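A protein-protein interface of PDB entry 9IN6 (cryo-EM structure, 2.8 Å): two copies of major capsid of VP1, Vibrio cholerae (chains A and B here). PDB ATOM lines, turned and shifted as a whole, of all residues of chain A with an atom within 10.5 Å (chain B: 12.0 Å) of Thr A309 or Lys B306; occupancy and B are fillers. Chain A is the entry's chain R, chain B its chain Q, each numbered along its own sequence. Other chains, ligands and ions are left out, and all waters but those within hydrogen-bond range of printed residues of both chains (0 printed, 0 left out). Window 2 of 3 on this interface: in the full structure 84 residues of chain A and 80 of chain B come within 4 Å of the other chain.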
ATOM      1  N   ARG A 295     -16.805  11.415  23.658  1.00  0.00           N
ATOM      2  CA  ARG A 295     -16.517  11.933  22.324  1.00  0.00           C
ATOM      3  C   ARG A 295     -15.366  11.187  21.663  1.00  0.00           C
ATOM      4  O   ARG A 295     -15.381  10.967  20.449  1.00  0.00           O
ATOM      5  CB  ARG A 295     -16.205  13.427  22.398  1.00  0.00           C
ATOM      6  CG  ARG A 295     -16.059  14.094  21.046  1.00  0.00           C
ATOM      7  CD  ARG A 295     -15.263  15.377  21.156  1.00  0.00           C
ATOM      8  NE  ARG A 295     -13.835  15.121  21.277  1.00  0.00           N
ATOM      9  CZ  ARG A 295     -12.962  15.983  21.775  1.00  0.00           C
ATOM     10  NH1 ARG A 295     -13.340  17.168  22.222  1.00  0.00           N
ATOM     11  NH2 ARG A 295     -11.677  15.646  21.830  1.00  0.00           N
ATOM     12  N   THR A 300     -18.058   6.692  17.975  1.00  0.00           N
ATOM     13  CA  THR A 300     -18.896   7.879  18.082  1.00  0.00           C
ATOM     14  C   THR A 300     -18.580   8.836  16.942  1.00  0.00           C
ATOM     15  O   THR A 300     -17.409   9.105  16.665  1.00  0.00           O
ATOM     16  CB  THR A 300     -18.682   8.576  19.424  1.00  0.00           C
ATOM     17  OG1 THR A 300     -19.003   7.672  20.486  1.00  0.00           O
ATOM     18  CG2 THR A 300     -19.562   9.802  19.531  1.00  0.00           C
ATOM     19  N   ARG A 301     -19.621   9.343  16.282  1.00  0.00           N
ATOM     20  CA  ARG A 301     -19.456  10.301  15.199  1.00  0.00           C
ATOM     21  C   ARG A 301     -20.480  11.421  15.307  1.00  0.00           C
ATOM     22  O   ARG A 301     -21.538  11.279  15.922  1.00  0.00           O
ATOM     23  CB  ARG A 301     -19.553   9.640  13.817  1.00  0.00           C
ATOM     24  CG  ARG A 301     -18.282   8.940  13.381  1.00  0.00           C
ATOM     25  CD  ARG A 301     -18.178   7.540  13.907  1.00  0.00           C
ATOM     26  NE  ARG A 301     -17.060   6.828  13.302  1.00  0.00           N
ATOM     27  CZ  ARG A 301     -15.846   6.765  13.829  1.00  0.00           C
ATOM     28  NH1 ARG A 301     -15.559   7.361  14.972  1.00  0.00           N
ATOM     29  NH2 ARG A 301     -14.898   6.083  13.195  1.00  0.00           N
ATOM     30  N   ILE A 302     -20.130  12.551  14.695  1.00  0.00           N
ATOM     31  CA  ILE A 302     -20.964  13.742  14.627  1.00  0.00           C
ATOM     32  C   ILE A 302     -21.202  14.058  13.158  1.00  0.00           C
ATOM     33  O   ILE A 302     -20.250  14.140  12.375  1.00  0.00           O
ATOM     34  CB  ILE A 302     -20.291  14.925  15.349  1.00  0.00           C
ATOM     35  CG1 ILE A 302     -19.907  14.525  16.769  1.00  0.00           C
ATOM     36  CG2 ILE A 302     -21.199  16.123  15.379  1.00  0.00           C
ATOM     37  CD1 ILE A 302     -19.216  15.615  17.533  1.00  0.00           C
ATOM     38  N   ASN A 303     -22.466  14.232  12.779  1.00  0.00           N
ATOM     39  CA  ASN A 303     -22.872  14.172  11.377  1.00  0.00           C
ATOM     40  C   ASN A 303     -23.385  15.519  10.891  1.00  0.00           C
ATOM     41  O   ASN A 303     -24.347  16.058  11.441  1.00  0.00           O
ATOM     42  CB  ASN A 303     -23.946  13.104  11.180  1.00  0.00           C
ATOM     43  CG  ASN A 303     -23.465  11.723  11.554  1.00  0.00           C
ATOM     44  OD1 ASN A 303     -24.186  10.953  12.180  1.00  0.00           O
ATOM     45  ND2 ASN A 303     -22.242  11.399  11.168  1.00  0.00           N
ATOM     46  N   PHE A 304     -22.789  16.027   9.819  1.00  0.00           N
ATOM     47  CA  PHE A 304     -23.261  17.232   9.162  1.00  0.00           C
ATOM     48  C   PHE A 304     -23.737  16.900   7.754  1.00  0.00           C
ATOM     49  O   PHE A 304     -23.235  15.971   7.117  1.00  0.00           O
ATOM     50  CB  PHE A 304     -22.164  18.295   9.104  1.00  0.00           C
ATOM     51  CG  PHE A 304     -21.819  18.881  10.440  1.00  0.00           C
ATOM     52  CD1 PHE A 304     -22.563  19.916  10.969  1.00  0.00           C
ATOM     53  CD2 PHE A 304     -20.748  18.399  11.165  1.00  0.00           C
ATOM     54  CE1 PHE A 304     -22.249  20.455  12.197  1.00  0.00           C
ATOM     55  CE2 PHE A 304     -20.428  18.937  12.392  1.00  0.00           C
ATOM     56  CZ  PHE A 304     -21.179  19.967  12.906  1.00  0.00           C
ATOM     57  N   ASP A 305     -24.713  17.663   7.271  1.00  0.00           N
ATOM     58  CA  ASP A 305     -25.240  17.484   5.923  1.00  0.00           C
ATOM     59  C   ASP A 305     -24.607  18.490   4.975  1.00  0.00           C
ATOM     60  O   ASP A 305     -24.972  19.670   4.977  1.00  0.00           O
ATOM     61  CB  ASP A 305     -26.759  17.627   5.902  1.00  0.00           C
ATOM     62  CG  ASP A 305     -27.457  16.479   6.582  1.00  0.00           C
ATOM     63  OD1 ASP A 305     -26.758  15.599   7.121  1.00  0.00           O
ATOM     64  OD2 ASP A 305     -28.705  16.449   6.572  1.00  0.00           O
ATOM     65  N   LYS A 306     -23.633  18.024   4.193  1.00  0.00           N
ATOM     66  CA  LYS A 306     -23.058  18.737   3.060  1.00  0.00           C
ATOM     67  C   LYS A 306     -22.176  19.910   3.464  1.00  0.00           C
ATOM     68  O   LYS A 306     -21.448  20.445   2.625  1.00  0.00           O
ATOM     69  CB  LYS A 306     -24.159  19.247   2.128  1.00  0.00           C
ATOM     70  CG  LYS A 306     -25.055  18.191   1.532  1.00  0.00           C
ATOM     71  CD  LYS A 306     -26.318  18.826   0.988  1.00  0.00           C
ATOM     72  CE  LYS A 306     -27.133  17.846   0.175  1.00  0.00           C
ATOM     73  NZ  LYS A 306     -26.410  17.434  -1.053  1.00  0.00           N
ATOM     74  N   GLN A 307     -22.201  20.299   4.737  1.00  0.00           N
ATOM     75  CA  GLN A 307     -21.449  21.458   5.192  1.00  0.00           C
ATOM     76  C   GLN A 307     -21.526  21.569   6.705  1.00  0.00           C
ATOM     77  O   GLN A 307     -22.561  21.289   7.312  1.00  0.00           O
ATOM     78  CB  GLN A 307     -21.968  22.757   4.564  1.00  0.00           C
ATOM     79  CG  GLN A 307     -23.440  23.008   4.800  1.00  0.00           C
ATOM     80  CD  GLN A 307     -23.913  24.296   4.167  1.00  0.00           C
ATOM     81  OE1 GLN A 307     -23.116  25.069   3.648  1.00  0.00           O
ATOM     82  NE2 GLN A 307     -25.216  24.530   4.206  1.00  0.00           N
ATOM     83  N   VAL A 308     -20.420  21.993   7.309  1.00  0.00           N
ATOM     84  CA  VAL A 308     -20.418  22.319   8.729  1.00  0.00           C
ATOM     85  C   VAL A 308     -21.125  23.654   8.913  1.00  0.00           C
ATOM     86  O   VAL A 308     -20.758  24.655   8.290  1.00  0.00           O
ATOM     87  CB  VAL A 308     -18.989  22.369   9.276  1.00  0.00           C
ATOM     88  CG1 VAL A 308     -19.008  22.657  10.760  1.00  0.00           C
ATOM     89  CG2 VAL A 308     -18.270  21.071   8.991  1.00  0.00           C
ATOM     90  N   THR A 309     -22.144  23.677   9.767  1.00  0.00           N
ATOM     91  CA  THR A 309     -22.948  24.879   9.914  1.00  0.00           C
ATOM     92  C   THR A 309     -23.567  24.933  11.303  1.00  0.00           C
ATOM     93  O   THR A 309     -23.652  23.927  12.010  1.00  0.00           O
ATOM     94  CB  THR A 309     -24.037  24.949   8.838  1.00  0.00           C
ATOM     95  OG1 THR A 309     -24.611  26.258   8.817  1.00  0.00           O
ATOM     96  CG2 THR A 309     -25.126  23.939   9.117  1.00  0.00           C
ATOM     97  N   GLN A 310     -23.971  26.144  11.688  1.00  0.00           N
ATOM     98  CA  GLN A 310     -24.715  26.445  12.910  1.00  0.00           C
ATOM     99  C   GLN A 310     -23.914  26.289  14.196  1.00  0.00           C
ATOM    100  O   GLN A 310     -23.528  27.290  14.803  1.00  0.00           O
ATOM    101  CB  GLN A 310     -25.981  25.594  12.991  1.00  0.00           C
ATOM    102  CG  GLN A 310     -27.015  25.964  11.957  1.00  0.00           C
ATOM    103  CD  GLN A 310     -28.239  25.082  12.020  1.00  0.00           C
ATOM    104  OE1 GLN A 310     -28.526  24.471  13.050  1.00  0.00           O
ATOM    105  NE2 GLN A 310     -28.971  25.009  10.916  1.00  0.00           N
ATOM    106  N   VAL A 311     -23.654  25.057  14.634  1.00  0.00           N
ATOM    107  CA  VAL A 311     -23.147  24.828  15.982  1.00  0.00           C
ATOM    108  C   VAL A 311     -22.220  23.623  15.969  1.00  0.00           C
ATOM    109  O   VAL A 311     -22.285  22.780  15.078  1.00  0.00           O
ATOM    110  CB  VAL A 311     -24.315  24.635  16.982  1.00  0.00           C
ATOM    111  CG1 VAL A 311     -24.959  23.282  16.792  1.00  0.00           C
ATOM    112  CG2 VAL A 311     -23.841  24.817  18.407  1.00  0.00           C
ATOM    113  N   TYR A 312     -21.340  23.554  16.966  1.00  0.00           N
ATOM    114  CA  TYR A 312     -20.450  22.425  17.175  1.00  0.00           C
ATOM    115  C   TYR A 312     -20.038  22.402  18.638  1.00  0.00           C
ATOM    116  O   TYR A 312     -19.930  23.452  19.274  1.00  0.00           O
ATOM    117  CB  TYR A 312     -19.212  22.514  16.281  1.00  0.00           C
ATOM    118  CG  TYR A 312     -18.181  21.456  16.567  1.00  0.00           C
ATOM    119  CD1 TYR A 312     -18.390  20.140  16.193  1.00  0.00           C
ATOM    120  CD2 TYR A 312     -17.008  21.768  17.224  1.00  0.00           C
ATOM    121  CE1 TYR A 312     -17.454  19.169  16.456  1.00  0.00           C
ATOM    122  CE2 TYR A 312     -16.067  20.802  17.493  1.00  0.00           C
ATOM    123  CZ  TYR A 312     -16.295  19.507  17.104  1.00  0.00           C
ATOM    124  OH  TYR A 312     -15.356  18.543  17.371  1.00  0.00           O
ATOM    125  N   GLY A 313     -19.809  21.210  19.168  1.00  0.00           N
ATOM    126  CA  GLY A 313     -19.352  21.074  20.531  1.00  0.00           C
ATOM    127  C   GLY A 313     -19.942  19.847  21.188  1.00  0.00           C
ATOM    128  O   GLY A 313     -20.313  18.882  20.525  1.00  0.00           O
ATOM    129  N   MET A 314     -20.025  19.888  22.518  1.00  0.00           N
ATOM    130  CA  MET A 314     -20.521  18.755  23.289  1.00  0.00           C
ATOM    131  C   MET A 314     -20.941  19.200  24.683  1.00  0.00           C
ATOM    132  O   MET A 314     -20.198  19.913  25.361  1.00  0.00           O
ATOM    133  CB  MET A 314     -19.457  17.656  23.384  1.00  0.00           C
ATOM    134  CG  MET A 314     -18.214  18.051  24.163  1.00  0.00           C
ATOM    135  SD  MET A 314     -16.953  16.774  24.224  1.00  0.00           S
ATOM    136  CE  MET A 314     -15.696  17.613  25.179  1.00  0.00           C
ATOM    137  N   ASN A 315     -22.151  18.813  25.089  1.00  0.00           N
ATOM    138  CA  ASN A 315     -22.544  18.862  26.492  1.00  0.00           C
ATOM    139  C   ASN A 315     -23.716  17.929  26.772  1.00  0.00           C
ATOM    140  O   ASN A 315     -24.866  18.270  26.483  1.00  0.00           O
ATOM    141  CB  ASN A 315     -22.894  20.290  26.916  1.00  0.00           C
ATOM    142  CG  ASN A 315     -23.906  20.939  26.007  1.00  0.00           C
ATOM    143  OD1 ASN A 315     -24.232  20.411  24.949  1.00  0.00           O
ATOM    144  ND2 ASN A 315     -24.425  22.083  26.425  1.00  0.00           N
ATOM    145  N   ILE B 302     -22.358   5.091  16.794  1.00  0.00           N
ATOM    146  CA  ILE B 302     -23.331   5.895  17.527  1.00  0.00           C
ATOM    147  C   ILE B 302     -23.234   7.317  16.993  1.00  0.00           C
ATOM    148  O   ILE B 302     -22.152   7.914  17.006  1.00  0.00           O
ATOM    149  CB  ILE B 302     -23.083   5.850  19.040  1.00  0.00           C
ATOM    150  CG1 ILE B 302     -23.137   4.408  19.537  1.00  0.00           C
ATOM    151  CG2 ILE B 302     -24.104   6.689  19.769  1.00  0.00           C
ATOM    152  CD1 ILE B 302     -22.641   4.231  20.943  1.00  0.00           C
ATOM    153  N   ASN B 303     -24.360   7.863  16.536  1.00  0.00           N
ATOM    154  CA  ASN B 303     -24.362   9.047  15.679  1.00  0.00           C
ATOM    155  C   ASN B 303     -25.121  10.200  16.323  1.00  0.00           C
ATOM    156  O   ASN B 303     -26.355  10.230  16.292  1.00  0.00           O
ATOM    157  CB  ASN B 303     -24.976   8.716  14.320  1.00  0.00           C
ATOM    158  CG  ASN B 303     -24.236   7.620  13.600  1.00  0.00           C
ATOM    159  OD1 ASN B 303     -24.842   6.689  13.084  1.00  0.00           O
ATOM    160  ND2 ASN B 303     -22.917   7.730  13.552  1.00  0.00           N
ATOM    161  N   PHE B 304     -24.391  11.176  16.848  1.00  0.00           N
ATOM    162  CA  PHE B 304     -24.975  12.457  17.211  1.00  0.00           C
ATOM    163  C   PHE B 304     -24.964  13.377  15.999  1.00  0.00           C
ATOM    164  O   PHE B 304     -24.116  13.252  15.113  1.00  0.00           O
ATOM    165  CB  PHE B 304     -24.210  13.101  18.365  1.00  0.00           C
ATOM    166  CG  PHE B 304     -24.120  12.237  19.579  1.00  0.00           C
ATOM    167  CD1 PHE B 304     -23.048  11.388  19.761  1.00  0.00           C
ATOM    168  CD2 PHE B 304     -25.115  12.263  20.534  1.00  0.00           C
ATOM    169  CE1 PHE B 304     -22.967  10.590  20.875  1.00  0.00           C
ATOM    170  CE2 PHE B 304     -25.038  11.465  21.647  1.00  0.00           C
ATOM    171  CZ  PHE B 304     -23.964  10.629  21.819  1.00  0.00           C
ATOM    172  N   ASP B 305     -25.920  14.306  15.957  1.00  0.00           N
ATOM    173  CA  ASP B 305     -26.051  15.149  14.773  1.00  0.00           C
ATOM    174  C   ASP B 305     -24.970  16.220  14.730  1.00  0.00           C
ATOM    175  O   ASP B 305     -24.044  16.150  13.918  1.00  0.00           O
ATOM    176  CB  ASP B 305     -27.435  15.790  14.736  1.00  0.00           C
ATOM    177  CG  ASP B 305     -28.453  14.924  14.036  1.00  0.00           C
ATOM    178  OD1 ASP B 305     -28.085  13.817  13.598  1.00  0.00           O
ATOM    179  OD2 ASP B 305     -29.619  15.349  13.918  1.00  0.00           O
ATOM    180  N   LYS B 306     -25.019  17.179  15.642  1.00  0.00           N
ATOM    181  CA  LYS B 306     -24.053  18.268  15.617  1.00  0.00           C
ATOM    182  C   LYS B 306     -23.293  18.441  16.914  1.00  0.00           C
ATOM    183  O   LYS B 306     -22.306  19.184  16.930  1.00  0.00           O
ATOM    184  CB  LYS B 306     -24.740  19.594  15.271  1.00  0.00           C
ATOM    185  CG  LYS B 306     -25.411  19.607  13.917  1.00  0.00           C
ATOM    186  CD  LYS B 306     -25.697  21.024  13.473  1.00  0.00           C
ATOM    187  CE  LYS B 306     -26.379  21.053  12.126  1.00  0.00           C
ATOM    188  NZ  LYS B 306     -27.846  20.896  12.265  1.00  0.00           N
ATOM    189  N   GLN B 307     -23.706  17.784  17.991  1.00  0.00           N
ATOM    190  CA  GLN B 307     -23.095  17.963  19.295  1.00  0.00           C
ATOM    191  C   GLN B 307     -23.525  16.812  20.184  1.00  0.00           C
ATOM    192  O   GLN B 307     -24.687  16.405  20.157  1.00  0.00           O
ATOM    193  CB  GLN B 307     -23.509  19.299  19.911  1.00  0.00           C
ATOM    194  CG  GLN B 307     -24.979  19.601  19.716  1.00  0.00           C
ATOM    195  CD  GLN B 307     -25.383  20.933  20.291  1.00  0.00           C
ATOM    196  OE1 GLN B 307     -24.644  21.541  21.062  1.00  0.00           O
ATOM    197  NE2 GLN B 307     -26.556  21.409  19.903  1.00  0.00           N
ATOM    198  N   VAL B 308     -22.587  16.291  20.965  1.00  0.00           N
ATOM    199  CA  VAL B 308     -22.927  15.279  21.953  1.00  0.00           C
ATOM    200  C   VAL B 308     -23.740  15.994  23.017  1.00  0.00           C
ATOM    201  O   VAL B 308     -23.187  16.741  23.828  1.00  0.00           O
ATOM    202  CB  VAL B 308     -21.665  14.628  22.541  1.00  0.00           C
ATOM    203  CG1 VAL B 308     -22.036  13.639  23.616  1.00  0.00           C
ATOM    204  CG2 VAL B 308     -20.849  13.977  21.451  1.00  0.00           C
ATOM    205  N   THR B 309     -25.053  15.795  23.018  1.00  0.00           N
ATOM    206  CA  THR B 309     -25.905  16.751  23.713  1.00  0.00           C
ATOM    207  C   THR B 309     -26.842  16.154  24.750  1.00  0.00           C
ATOM    208  O   THR B 309     -27.038  16.765  25.800  1.00  0.00           O
ATOM    209  CB  THR B 309     -26.730  17.551  22.693  1.00  0.00           C
ATOM    210  OG1 THR B 309     -27.644  18.407  23.385  1.00  0.00           O
ATOM    211  CG2 THR B 309     -27.502  16.624  21.776  1.00  0.00           C
ATOM    212  N   GLN B 310     -27.451  14.997  24.506  1.00  0.00           N
ATOM    213  CA  GLN B 310     -28.541  14.551  25.364  1.00  0.00           C
ATOM    214  C   GLN B 310     -28.212  13.299  26.162  1.00  0.00           C
ATOM    215  O   GLN B 310     -28.240  13.324  27.394  1.00  0.00           O
ATOM    216  CB  GLN B 310     -29.793  14.304  24.520  1.00  0.00           C
ATOM    217  CG  GLN B 310     -30.691  15.500  24.365  1.00  0.00           C
ATOM    218  CD  GLN B 310     -31.972  15.150  23.644  1.00  0.00           C
ATOM    219  OE1 GLN B 310     -32.574  14.107  23.894  1.00  0.00           O
ATOM    220  NE2 GLN B 310     -32.400  16.026  22.745  1.00  0.00           N
ATOM    221  N   VAL B 311     -27.905  12.194  25.490  1.00  0.00           N
ATOM    222  CA  VAL B 311     -27.828  10.888  26.128  1.00  0.00           C
ATOM    223  C   VAL B 311     -26.633  10.141  25.561  1.00  0.00           C
ATOM    224  O   VAL B 311     -26.250  10.344  24.406  1.00  0.00           O
ATOM    225  CB  VAL B 311     -29.124  10.072  25.915  1.00  0.00           C
ATOM    226  CG1 VAL B 311     -29.129   8.843  26.787  1.00  0.00           C
ATOM    227  CG2 VAL B 311     -30.355  10.910  26.201  1.00  0.00           C
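N of Phe B304 sits at hydrogen-bond distance from O of Arg A301, at 3.0 Å. N of Asn A303 is in hydrogen-bond range of O of Asp B305. O of Thr B309 lies close to O of Asn A315, at 2.7 Å. The backbone carbonyl oxygen (O) of Phe B304 is in hydrogen-bond range of the backbone NH (N) of Asn A303 (3.0 Å). The backbone NH (N) of Arg A301 sits at hydrogen-bond distance from the backbone carbonyl oxygen (O) of Ile B302 (3.0 Å). N of Val B308 sits at hydrogen-bond distance from O of Gly A313, at 3.5 Å. The backbone carbonyl oxygen of Val B308 lies within hydrogen-bond range of the backbone NH of Asn A315 (2.6 Å).
Among the printed residues, merely in contact across the chains: Thr A300 with Ile B302 (3.4 Å), Thr A300 with Phe B304 (3.7 Å), Arg A301 with Asn B303 (3.6 Å), Ile A302 with Phe B304 (3.2 Å), Ile A302 with Asp B305 (3.2 Å), Ile A302 with Lys B306 (3.5 Å), Ile A302 with Gln B307 (3.98 Å), Asn A303 with Asn B303 (3.2 Å), Phe A304 with Lys B306 (3.7 Å), Thr A309 with Lys B306 (3.8 Å), Gln A310 with Lys B306 (3.7 Å), Val A311 with Lys B306 (3.995 Å), Val A311 with Gln B307 (3.97 Å), Tyr A312 with Lys B306 (3.7 Å), Gly A313 with Lys B306 (3.9 Å), Gly A313 with Gln B307 (3.2 Å) and Met A314 with Val B308 (3.4 Å).
Arg A295 touches none of the printed residues of chain B. Of the printed residues of chain B, Arg A301 touches Ile B302 (3.0 Å), Asn B303 (3.6 Å) and Phe B304 (3.0 Å). Of the printed residues of chain B, Ile A302 touches Phe B304, Asp B305, Lys B306 and Gln B307. Phe A304 touches just one residue of chain B: Lys B306. No residue of chain B comes within 4 Å of Asp A305. No residue of chain B comes within 4 Å of Gln A307. No residue of chain B comes within 4 Å of Val A308. Thr A309 touches one residue of chain B. Of the printed residues of chain B, Tyr A312 touches Lys B306. Of chain B, only Lys B306, Gln B307 and Val B308 come within 4 Å of Gly A313. Printed residues of chain A within 4 Å of Lys B306: Ile A302 (3.5 Å), Phe A304 (3.7 Å), Thr A309 (3.8 Å), Gln A310 (3.7 Å), Val A311 (3.995 Å), Tyr A312 (3.7 Å) and Gly A313 (3.9 Å). Of the printed residues of chain A, Val B308 touches Gly A313 (3.5 Å), Met A314 (3.4 Å) and Asn A315 (2.6 Å). Gln B310 touches none of the printed residues of chain A. The nearest printed residue of chain A that does not touch Lys B306 is Asn A303 (4.4 Å).
Of the 10 printed residues of chain B, 8 touch a printed residue of chain A. Printed residues of chain B that touch a printed residue of chain A: Ile B302, Asn B303, Phe B304, Asp B305, Lys B306, Gln B307, Val B308 and Thr B309. Along chain B the printed residues that touch a printed residue of chain A span positions 302 to 309. Among the printed residues, 24 pairs touch across the chains. Among the printed residues, no Asp or Glu carboxylate lies within 4 Å of a Lys or Arg side-chain nitrogen of the other chain.
Ile A302 touches Gln B307, but with the chains exchanged Gln A307 does not touch Ile B302 (16.5 Å). Phe A304 touches Lys B306, but with the chains exchanged Lys A306 does not touch Phe B304 (11.9 Å). Thr A309 touches Lys B306, but with the chains exchanged Lys A306 does not touch Thr B309 (18.1 Å). Val A311 touches Gln B307, but with the chains exchanged Gln A307 does not touch Val B311 (20.6 Å). Of the 24 pairs that touch across the chains among the printed residues, 1 has its exchanged pair printed and touching as well.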
